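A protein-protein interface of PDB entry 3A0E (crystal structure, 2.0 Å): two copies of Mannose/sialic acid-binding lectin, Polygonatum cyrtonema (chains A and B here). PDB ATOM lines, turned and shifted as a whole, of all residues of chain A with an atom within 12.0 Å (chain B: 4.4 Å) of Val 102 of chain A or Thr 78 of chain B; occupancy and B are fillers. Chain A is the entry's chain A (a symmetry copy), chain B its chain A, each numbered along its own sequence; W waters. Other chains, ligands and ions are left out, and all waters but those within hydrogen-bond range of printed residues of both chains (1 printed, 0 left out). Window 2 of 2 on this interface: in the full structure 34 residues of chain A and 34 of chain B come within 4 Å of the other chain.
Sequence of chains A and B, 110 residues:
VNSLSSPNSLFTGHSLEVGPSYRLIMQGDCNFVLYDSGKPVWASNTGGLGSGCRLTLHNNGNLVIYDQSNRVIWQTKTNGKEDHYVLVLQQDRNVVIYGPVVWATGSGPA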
ATOM      1  N   SER A   5      32.123 -26.239  -8.810  1.00  0.00           N
ATOM      2  CA  SER A   5      31.359 -25.001  -8.755  1.00  0.00           C
ATOM      3  C   SER A   5      32.117 -23.834  -9.379  1.00  0.00           C
ATOM      4  O   SER A   5      33.322 -23.683  -9.171  1.00  0.00           O
ATOM      5  CB  SER A   5      31.008 -24.670  -7.301  1.00  0.00           C
ATOM      6  OG  SER A   5      30.216 -25.697  -6.728  1.00  0.00           O
ATOM      7  N   SER A   6      31.407 -23.012 -10.146  1.00  0.00           N
ATOM      8  CA  SER A   6      32.030 -21.853 -10.781  1.00  0.00           C
ATOM      9  C   SER A   6      32.540 -20.937  -9.674  1.00  0.00           C
ATOM     10  O   SER A   6      31.970 -20.896  -8.580  1.00  0.00           O
ATOM     11  CB  SER A   6      31.011 -21.103 -11.652  1.00  0.00           C
ATOM     12  OG  SER A   6      29.984 -20.523 -10.864  1.00  0.00           O
ATOM     13  N   ASN A  59      31.252 -18.220 -14.026  1.00  0.00           N
ATOM     14  CA  ASN A  59      30.119 -17.708 -13.268  1.00  0.00           C
ATOM     15  C   ASN A  59      28.924 -17.302 -14.124  1.00  0.00           C
ATOM     16  O   ASN A  59      27.932 -16.793 -13.605  1.00  0.00           O
ATOM     17  CB  ASN A  59      30.546 -16.532 -12.380  1.00  0.00           C
ATOM     18  CG  ASN A  59      31.368 -16.980 -11.183  1.00  0.00           C
ATOM     19  OD1 ASN A  59      31.211 -18.102 -10.697  1.00  0.00           O
ATOM     20  ND2 ASN A  59      32.236 -16.098 -10.693  1.00  0.00           N
ATOM     21  N   LYS A  81      23.212 -15.523 -17.481  1.00  0.00           N
ATOM     22  CA  LYS A  81      23.274 -14.486 -16.463  1.00  0.00           C
ATOM     23  C   LYS A  81      24.456 -14.673 -15.516  1.00  0.00           C
ATOM     24  O   LYS A  81      24.823 -15.799 -15.171  1.00  0.00           O
ATOM     25  CB  LYS A  81      21.966 -14.469 -15.664  1.00  0.00           C
ATOM     26  CG  LYS A  81      21.884 -13.363 -14.626  1.00  0.00           C
ATOM     27  CD  LYS A  81      21.902 -13.911 -13.208  1.00  0.00           C
ATOM     28  CE  LYS A  81      20.651 -14.719 -12.905  1.00  0.00           C
ATOM     29  NZ  LYS A  81      20.675 -15.250 -11.513  1.00  0.00           N
ATOM     30  N   GLU A  82      25.049 -13.557 -15.107  1.00  0.00           N
ATOM     31  CA  GLU A  82      26.181 -13.568 -14.189  1.00  0.00           C
ATOM     32  C   GLU A  82      25.655 -13.956 -12.806  1.00  0.00           C
ATOM     33  O   GLU A  82      24.814 -13.261 -12.238  1.00  0.00           O
ATOM     34  CB  GLU A  82      26.820 -12.176 -14.151  1.00  0.00           C
ATOM     35  CG  GLU A  82      28.166 -12.105 -13.459  1.00  0.00           C
ATOM     36  CD  GLU A  82      29.169 -13.100 -14.015  1.00  0.00           C
ATOM     37  OE1 GLU A  82      29.192 -13.308 -15.248  1.00  0.00           O
ATOM     38  OE2 GLU A  82      29.941 -13.666 -13.213  1.00  0.00           O
ATOM     39  N   ASP A  83      26.152 -15.064 -12.269  1.00  0.00           N
ATOM     40  CA  ASP A  83      25.701 -15.557 -10.969  1.00  0.00           C
ATOM     41  C   ASP A  83      26.702 -16.646 -10.578  1.00  0.00           C
ATOM     42  O   ASP A  83      27.909 -16.405 -10.564  1.00  0.00           O
ATOM     43  CB  ASP A  83      24.288 -16.133 -11.138  1.00  0.00           C
ATOM     44  CG  ASP A  83      23.535 -16.263  -9.832  1.00  0.00           C
ATOM     45  OD1 ASP A  83      23.768 -17.241  -9.093  1.00  0.00           O
ATOM     46  OD2 ASP A  83      22.702 -15.378  -9.545  1.00  0.00           O
ATOM     47  N   HIS A  84      26.204 -17.833 -10.247  1.00  0.00           N
ATOM     48  CA  HIS A  84      27.070 -18.966  -9.930  1.00  0.00           C
ATOM     49  C   HIS A  84      26.415 -20.229 -10.462  1.00  0.00           C
ATOM     50  O   HIS A  84      25.189 -20.350 -10.473  1.00  0.00           O
ATOM     51  CB  HIS A  84      27.334 -19.093  -8.427  1.00  0.00           C
ATOM     52  CG  HIS A  84      28.338 -18.109  -7.913  1.00  0.00           C
ATOM     53  ND1 HIS A  84      27.978 -16.892  -7.379  1.00  0.00           N
ATOM     54  CD2 HIS A  84      29.692 -18.134  -7.915  1.00  0.00           C
ATOM     55  CE1 HIS A  84      29.067 -16.206  -7.078  1.00  0.00           C
ATOM     56  NE2 HIS A  84      30.121 -16.937  -7.394  1.00  0.00           N
ATOM     57  N   TYR A  85      27.242 -21.155 -10.929  1.00  0.00           N
ATOM     58  CA  TYR A  85      26.746 -22.401 -11.493  1.00  0.00           C
ATOM     59  C   TYR A  85      27.558 -23.579 -10.982  1.00  0.00           C
ATOM     60  O   TYR A  85      28.595 -23.401 -10.339  1.00  0.00           O
ATOM     61  CB  TYR A  85      26.822 -22.348 -13.023  1.00  0.00           C
ATOM     62  CG  TYR A  85      25.974 -21.253 -13.639  1.00  0.00           C
ATOM     63  CD1 TYR A  85      26.354 -19.912 -13.548  1.00  0.00           C
ATOM     64  CD2 TYR A  85      24.775 -21.554 -14.281  1.00  0.00           C
ATOM     65  CE1 TYR A  85      25.556 -18.895 -14.079  1.00  0.00           C
ATOM     66  CE2 TYR A  85      23.966 -20.546 -14.815  1.00  0.00           C
ATOM     67  CZ  TYR A  85      24.365 -19.221 -14.708  1.00  0.00           C
ATOM     68  OH  TYR A  85      23.573 -18.225 -15.228  1.00  0.00           O
ATOM     69  N   VAL A  86      27.080 -24.784 -11.268  1.00  0.00           N
ATOM     70  CA  VAL A  86      27.779 -25.985 -10.844  1.00  0.00           C
ATOM     71  C   VAL A  86      27.710 -27.053 -11.929  1.00  0.00           C
ATOM     72  O   VAL A  86      26.726 -27.142 -12.667  1.00  0.00           O
ATOM     73  CB  VAL A  86      27.182 -26.562  -9.532  1.00  0.00           C
ATOM     74  CG1 VAL A  86      25.776 -27.106  -9.781  1.00  0.00           C
ATOM     75  CG2 VAL A  86      28.094 -27.663  -8.987  1.00  0.00           C
ATOM     76  N   ILE A  97      25.210 -29.199 -16.054  1.00  0.00           N
ATOM     77  CA  ILE A  97      25.527 -27.867 -15.559  1.00  0.00           C
ATOM     78  C   ILE A  97      24.202 -27.279 -15.074  1.00  0.00           C
ATOM     79  O   ILE A  97      23.238 -27.205 -15.843  1.00  0.00           O
ATOM     80  CB  ILE A  97      26.074 -26.942 -16.668  1.00  0.00           C
ATOM     81  CG1 ILE A  97      27.432 -27.450 -17.161  1.00  0.00           C
ATOM     82  CG2 ILE A  97      26.200 -25.518 -16.130  1.00  0.00           C
ATOM     83  CD1 ILE A  97      28.016 -26.623 -18.291  1.00  0.00           C
ATOM     84  N   TYR A  98      24.152 -26.884 -13.803  1.00  0.00           N
ATOM     85  CA  TYR A  98      22.948 -26.288 -13.214  1.00  0.00           C
ATOM     86  C   TYR A  98      23.227 -24.870 -12.738  1.00  0.00           C
ATOM     87  O   TYR A  98      24.326 -24.567 -12.275  1.00  0.00           O
ATOM     88  CB  TYR A  98      22.465 -27.070 -11.991  1.00  0.00           C
ATOM     89  CG  TYR A  98      21.944 -28.457 -12.255  1.00  0.00           C
ATOM     90  CD1 TYR A  98      22.793 -29.562 -12.199  1.00  0.00           C
ATOM     91  CD2 TYR A  98      20.584 -28.674 -12.487  1.00  0.00           C
ATOM     92  CE1 TYR A  98      22.296 -30.855 -12.355  1.00  0.00           C
ATOM     93  CE2 TYR A  98      20.079 -29.963 -12.650  1.00  0.00           C
ATOM     94  CZ  TYR A  98      20.940 -31.046 -12.578  1.00  0.00           C
ATOM     95  OH  TYR A  98      20.442 -32.320 -12.710  1.00  0.00           O
ATOM     96  N   GLY A  99      22.211 -24.018 -12.815  1.00  0.00           N
ATOM     97  CA  GLY A  99      22.370 -22.644 -12.375  1.00  0.00           C
ATOM     98  C   GLY A  99      21.268 -21.777 -12.946  1.00  0.00           C
ATOM     99  O   GLY A  99      20.584 -22.202 -13.872  1.00  0.00           O
ATOM    100  N   PRO A 100      21.086 -20.547 -12.442  1.00  0.00           N
ATOM    101  CA  PRO A 100      21.858 -19.915 -11.369  1.00  0.00           C
ATOM    102  C   PRO A 100      21.493 -20.415  -9.971  1.00  0.00           C
ATOM    103  O   PRO A 100      20.823 -21.437  -9.816  1.00  0.00           O
ATOM    104  CB  PRO A 100      21.531 -18.440 -11.552  1.00  0.00           C
ATOM    105  CG  PRO A 100      20.089 -18.493 -11.938  1.00  0.00           C
ATOM    106  CD  PRO A 100      20.049 -19.626 -12.949  1.00  0.00           C
ATOM    107  N   VAL A 101      21.939 -19.679  -8.958  1.00  0.00           N
ATOM    108  CA  VAL A 101      21.665 -20.032  -7.571  1.00  0.00           C
ATOM    109  C   VAL A 101      20.194 -19.822  -7.217  1.00  0.00           C
ATOM    110  O   VAL A 101      19.618 -18.773  -7.499  1.00  0.00           O
ATOM    111  CB  VAL A 101      22.522 -19.189  -6.602  1.00  0.00           C
ATOM    112  CG1 VAL A 101      22.173 -19.539  -5.162  1.00  0.00           C
ATOM    113  CG2 VAL A 101      23.999 -19.443  -6.861  1.00  0.00           C
ATOM    114  N   VAL A 102      19.598 -20.832  -6.593  1.00  0.00           N
ATOM    115  CA  VAL A 102      18.203 -20.776  -6.186  1.00  0.00           C
ATOM    116  C   VAL A 102      18.089 -20.508  -4.688  1.00  0.00           C
ATOM    117  O   VAL A 102      17.187 -19.801  -4.238  1.00  0.00           O
ATOM    118  CB  VAL A 102      17.480 -22.110  -6.506  1.00  0.00           C
ATOM    119  CG1 VAL A 102      16.132 -22.170  -5.788  1.00  0.00           C
ATOM    120  CG2 VAL A 102      17.282 -22.245  -8.011  1.00  0.00           C
ATOM    121  N   TRP A 103      19.019 -21.073  -3.925  1.00  0.00           N
ATOM    122  CA  TRP A 103      19.018 -20.937  -2.471  1.00  0.00           C
ATOM    123  C   TRP A 103      20.376 -21.394  -1.943  1.00  0.00           C
ATOM    124  O   TRP A 103      21.050 -22.196  -2.579  1.00  0.00           O
ATOM    125  CB  TRP A 103      17.918 -21.833  -1.891  1.00  0.00           C
ATOM    126  CG  TRP A 103      17.847 -21.892  -0.391  1.00  0.00           C
ATOM    127  CD1 TRP A 103      17.158 -21.046   0.434  1.00  0.00           C
ATOM    128  CD2 TRP A 103      18.450 -22.878   0.460  1.00  0.00           C
ATOM    129  NE1 TRP A 103      17.289 -21.449   1.745  1.00  0.00           N
ATOM    130  CE2 TRP A 103      18.077 -22.569   1.788  1.00  0.00           C
ATOM    131  CE3 TRP A 103      19.266 -23.992   0.228  1.00  0.00           C
ATOM    132  CZ2 TRP A 103      18.495 -23.339   2.883  1.00  0.00           C
ATOM    133  CZ3 TRP A 103      19.680 -24.760   1.318  1.00  0.00           C
ATOM    134  CH2 TRP A 103      19.291 -24.427   2.629  1.00  0.00           C
ATOM    135  N   ALA A 104      20.770 -20.888  -0.779  1.00  0.00           N
ATOM    136  CA  ALA A 104      22.041 -21.274  -0.179  1.00  0.00           C
ATOM    137  C   ALA A 104      21.984 -21.096   1.332  1.00  0.00           C
ATOM    138  O   ALA A 104      21.319 -20.192   1.836  1.00  0.00           O
ATOM    139  CB  ALA A 104      23.180 -20.445  -0.761  1.00  0.00           C
ATOM    140  N   THR A 105      22.680 -21.968   2.051  1.00  0.00           N
ATOM    141  CA  THR A 105      22.704 -21.908   3.509  1.00  0.00           C
ATOM    142  C   THR A 105      23.579 -20.763   3.987  1.00  0.00           C
ATOM    143  O   THR A 105      23.326 -20.174   5.037  1.00  0.00           O
ATOM    144  CB  THR A 105      23.285 -23.188   4.111  1.00  0.00           C
ATOM    145  OG1 THR A 105      24.603 -23.389   3.587  1.00  0.00           O
ATOM    146  CG2 THR A 105      22.406 -24.390   3.788  1.00  0.00           C
ATOM    147  N   GLY A 106      24.616 -20.463   3.213  1.00  0.00           N
ATOM    148  CA  GLY A 106      25.532 -19.407   3.592  1.00  0.00           C
ATOM    149  C   GLY A 106      26.540 -19.925   4.605  1.00  0.00           C
ATOM    150  O   GLY A 106      27.204 -19.142   5.287  1.00  0.00           O
ATOM    151  N   ASN B  60      11.155 -28.465  -9.219  1.00  0.00           N
ATOM    152  CA  ASN B  60      10.844 -27.055  -9.399  1.00  0.00           C
ATOM    153  C   ASN B  60      11.784 -26.231  -8.518  1.00  0.00           C
ATOM    154  O   ASN B  60      11.658 -25.015  -8.429  1.00  0.00           O
ATOM    155  CB  ASN B  60       9.370 -26.767  -9.068  1.00  0.00           C
ATOM    156  CG  ASN B  60       9.083 -26.783  -7.580  1.00  0.00           C
ATOM    157  OD1 ASN B  60       9.761 -27.462  -6.813  1.00  0.00           O
ATOM    158  ND2 ASN B  60       8.053 -26.042  -7.168  1.00  0.00           N
ATOM    159  N   GLY B  61      12.730 -26.912  -7.873  1.00  0.00           N
ATOM    160  CA  GLY B  61      13.702 -26.232  -7.028  1.00  0.00           C
ATOM    161  C   GLY B  61      13.410 -26.142  -5.539  1.00  0.00           C
ATOM    162  O   GLY B  61      14.233 -25.629  -4.781  1.00  0.00           O
ATOM    163  N   ASN B  62      12.256 -26.636  -5.105  1.00  0.00           N
ATOM    164  CA  ASN B  62      11.910 -26.575  -3.689  1.00  0.00           C
ATOM    165  C   ASN B  62      12.532 -27.743  -2.925  1.00  0.00           C
ATOM    166  O   ASN B  62      12.450 -28.895  -3.356  1.00  0.00           O
ATOM    167  CB  ASN B  62      10.383 -26.570  -3.519  1.00  0.00           C
ATOM    168  CG  ASN B  62       9.949 -26.199  -2.108  1.00  0.00           C
ATOM    169  OD1 ASN B  62      10.558 -25.346  -1.465  1.00  0.00           O
ATOM    170  ND2 ASN B  62       8.876 -26.827  -1.629  1.00  0.00           N
ATOM    171  N   LEU B  63      13.166 -27.427  -1.797  1.00  0.00           N
ATOM    172  CA  LEU B  63      13.816 -28.423  -0.944  1.00  0.00           C
ATOM    173  C   LEU B  63      12.921 -28.626   0.278  1.00  0.00           C
ATOM    174  O   LEU B  63      12.570 -27.662   0.962  1.00  0.00           O
ATOM    175  CB  LEU B  63      15.201 -27.928  -0.506  1.00  0.00           C
ATOM    176  CG  LEU B  63      16.060 -28.903   0.308  1.00  0.00           C
ATOM    177  CD1 LEU B  63      16.399 -30.129  -0.540  1.00  0.00           C
ATOM    178  CD2 LEU B  63      17.335 -28.207   0.761  1.00  0.00           C
ATOM    179  N   THR B  76      12.326 -24.868   1.924  1.00  0.00           N
ATOM    180  CA  THR B  76      12.937 -23.613   1.506  1.00  0.00           C
ATOM    181  C   THR B  76      11.925 -22.717   0.792  1.00  0.00           C
ATOM    182  O   THR B  76      12.147 -21.515   0.644  1.00  0.00           O
ATOM    183  CB  THR B  76      14.121 -23.868   0.554  1.00  0.00           C
ATOM    184  OG1 THR B  76      13.677 -24.660  -0.554  1.00  0.00           O
ATOM    185  CG2 THR B  76      15.243 -24.602   1.279  1.00  0.00           C
ATOM    186  N   LYS B  77      10.818 -23.306   0.355  1.00  0.00           N
ATOM    187  CA  LYS B  77       9.779 -22.567  -0.356  1.00  0.00           C
ATOM    188  C   LYS B  77      10.330 -21.888  -1.606  1.00  0.00           C
ATOM    189  O   LYS B  77      10.030 -20.724  -1.879  1.00  0.00           O
ATOM    190  CB  LYS B  77       9.139 -21.518   0.560  1.00  0.00           C
ATOM    191  CG  LYS B  77       8.400 -22.111   1.747  1.00  0.00           C
ATOM    192  CD  LYS B  77       7.642 -21.047   2.522  1.00  0.00           C
ATOM    193  CE  LYS B  77       6.883 -21.655   3.692  1.00  0.00           C
ATOM    194  NZ  LYS B  77       6.109 -20.625   4.446  1.00  0.00           N
ATOM    195  N   THR B  78      11.143 -22.617  -2.362  1.00  0.00           N
ATOM    196  CA  THR B  78      11.716 -22.084  -3.586  1.00  0.00           C
ATOM    197  C   THR B  78      11.045 -22.785  -4.765  1.00  0.00           C
ATOM    198  O   THR B  78      11.611 -23.688  -5.382  1.00  0.00           O
ATOM    199  CB  THR B  78      13.256 -22.286  -3.614  1.00  0.00           C
ATOM    200  OG1 THR B  78      13.585 -23.606  -3.166  1.00  0.00           O
ATOM    201  CG2 THR B  78      13.937 -21.276  -2.698  1.00  0.00           C
ATOM    202  N   ASN B  79       9.818 -22.359  -5.057  1.00  0.00           N
ATOM    203  CA  ASN B  79       9.030 -22.937  -6.139  1.00  0.00           C
ATOM    204  C   ASN B  79       9.220 -22.163  -7.439  1.00  0.00           C
ATOM    205  O   ASN B  79       8.646 -21.088  -7.628  1.00  0.00           O
ATOM    206  CB  ASN B  79       7.553 -22.952  -5.739  1.00  0.00           C
ATOM    207  CG  ASN B  79       7.300 -23.777  -4.490  1.00  0.00           C
ATOM    208  OD1 ASN B  79       7.469 -24.997  -4.493  1.00  0.00           O
ATOM    209  ND2 ASN B  79       6.907 -23.112  -3.410  1.00  0.00           N
ATOM    210  N   GLY B  80      10.030 -22.717  -8.335  1.00  0.00           N
ATOM    211  CA  GLY B  80      10.289 -22.050  -9.598  1.00  0.00           C
ATOM    212  C   GLY B  80       9.816 -22.829 -10.808  1.00  0.00           C
ATOM    213  O   GLY B  80       8.858 -23.600 -10.737  1.00  0.00           O
ATOM    214  N   TYR B  85      16.875 -29.625 -10.810  1.00  0.00           N
ATOM    215  CA  TYR B  85      17.769 -28.863  -9.952  1.00  0.00           C
ATOM    216  C   TYR B  85      18.694 -29.792  -9.184  1.00  0.00           C
ATOM    217  O   TYR B  85      18.515 -31.012  -9.193  1.00  0.00           O
ATOM    218  CB  TYR B  85      16.954 -28.018  -8.967  1.00  0.00           C
ATOM    219  CG  TYR B  85      16.056 -26.995  -9.637  1.00  0.00           C
ATOM    220  CD1 TYR B  85      14.894 -27.386 -10.305  1.00  0.00           C
ATOM    221  CD2 TYR B  85      16.389 -25.643  -9.634  1.00  0.00           C
ATOM    222  CE1 TYR B  85      14.085 -26.454 -10.959  1.00  0.00           C
ATOM    223  CE2 TYR B  85      15.589 -24.699 -10.286  1.00  0.00           C
ATOM    224  CZ  TYR B  85      14.440 -25.114 -10.945  1.00  0.00           C
ATOM    225  OH  TYR B  85      13.652 -24.191 -11.590  1.00  0.00           O
ATOM    226  N   ILE B  97      21.528 -24.763  -3.753  1.00  0.00           N
ATOM    227  CA  ILE B  97      20.591 -25.342  -4.705  1.00  0.00           C
ATOM    228  C   ILE B  97      20.802 -24.577  -6.012  1.00  0.00           C
ATOM    229  O   ILE B  97      20.691 -23.347  -6.034  1.00  0.00           O
ATOM    230  CB  ILE B  97      19.121 -25.147  -4.276  1.00  0.00           C
ATOM    231  CG1 ILE B  97      18.831 -25.935  -2.996  1.00  0.00           C
ATOM    232  CG2 ILE B  97      18.195 -25.600  -5.404  1.00  0.00           C
ATOM    233  CD1 ILE B  97      17.416 -25.754  -2.478  1.00  0.00           C
ATOM    234  N   GLY B  99      19.951 -24.391 -10.363  1.00  0.00           N
ATOM    235  CA  GLY B  99      19.007 -24.812 -11.382  1.00  0.00           C
ATOM    236  C   GLY B  99      18.402 -23.607 -12.071  1.00  0.00           C
ATOM    237  O   GLY B  99      18.521 -22.497 -11.560  1.00  0.00           O
HETATM  238  O   HOH W   1      18.075 -33.392 -11.440  1.00  0.00           O
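Hydrophobic or aromatic side chains of chain A within 4 Å of the printed part of chain B: Tyr 98, Pro 100, Val 102 and Trp 103.
Among the printed residues, 10 pairs touch across the chains.
Among the printed residues, no Asp or Glu carboxylate lies within 4 Å of a Lys or Arg side-chain nitrogen of the other chain.
Of the printed residues of chain B, Val 101 of chain A touches Ile 97.
Val 102 of chain A touches just these residues of chain B: Thr 78 (3.6 Å), Tyr 85 (3.8 Å), Ile 97 (2.8 Å) and Gly 99 (3.8 Å).
No residue of chain A comes within 4 Å of Asn 60 of chain B.
No residue of chain A comes within 4 Å of Gly 61 of chain B.
No residue of chain A comes within 4 Å of Leu 63 of chain B.
Thr 76 of chain B touches just one residue of chain A: Trp 103 (3.5 Å).
Of chain A, only Val 102 comes within 4 Å of Thr 78 of chain B.
No residue of chain A comes within 4 Å of Gly 80 of chain B.
Printed residues of chain A within 4 Å of Tyr 85 of chain B: Tyr 98 and Val 102.
Ile 97 of chain B touches just these residues of chain A: Val 101 (3.8 Å), Val 102 (2.8 Å) and Trp 103 (2.9 Å).
The nearest printed residue of chain B that does not touch Trp 103 of chain A is Thr 78 of chain B (4.1 Å).
Gly 99 of chain B touches its own counterpart, Gly 99 of chain A.
Of the 10 pairs that touch across the chains among the printed residues, 1 has its exchanged pair printed and touching as well.
The backbone carbonyl oxygen (O) of Ile 97 of chain B sits at hydrogen-bond distance from the backbone NH (N) of Val 102 of chain A, at 2.8 Å.
O of Pro 100 of chain A is in hydrogen-bond range of N of Gly 99 of chain B (3.1 Å).
The backbone carbonyl oxygen of Trp 103 of chain A lies within hydrogen-bond range of the backbone NH of Ile 97 of chain B, at 2.9 Å.
O of Gly 99 of chain A sits close to O of Gly 99 of chain B (3.1 Å).
Among the printed residues, pairs that only touch across the chains: Trp 103 of chain A with Thr 76 of chain B (3.5 Å), Val 102 of chain A with Thr 78 of chain B (3.6 Å), Tyr 98 of chain A with Tyr 85 of chain B (3.7 Å), Val 102 of chain A with Tyr 85 of chain B (3.8 Å), Val 101 of chain A with Ile 97 of chain B (3.8 Å) and Val 102 of chain A with Gly 99 of chain B (3.8 Å).
The backbone NH (N) of Val 101 of chain A sits at hydrogen-bond distance from the side-chain carboxylate (OD1) of Asp 83 of chain A (3.1 Å).
The side-chain hydroxyl (OG1) of Thr 78 of chain B lies within hydrogen-bond range of the backbone carbonyl oxygen (O) of Gly 61 of chain B (2.7 Å).
The backbone carbonyl oxygen (O) of Leu 63 of chain B lies within hydrogen-bond range of the backbone NH (N) of Thr 76 of chain B (3.0 Å).
The backbone NH of Tyr 98 of chain A lies within hydrogen-bond range of the backbone carbonyl oxygen of Val 86 of chain A (2.8 Å).
OD1 of Asn 62 of chain B lies within hydrogen-bond range of OG1 of Thr 76 of chain B (3.3 Å).
The side-chain amide oxygen (OD1) of Asn 62 of chain B lies within hydrogen-bond range of the backbone NH (N) of Thr 78 of chain B.
Water W1 lies within hydrogen-bond range of the side-chain hydroxyl of Tyr 98 of chain A (2.9 Å) and the backbone carbonyl oxygen of Tyr 85 of chain B (3.3 Å).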
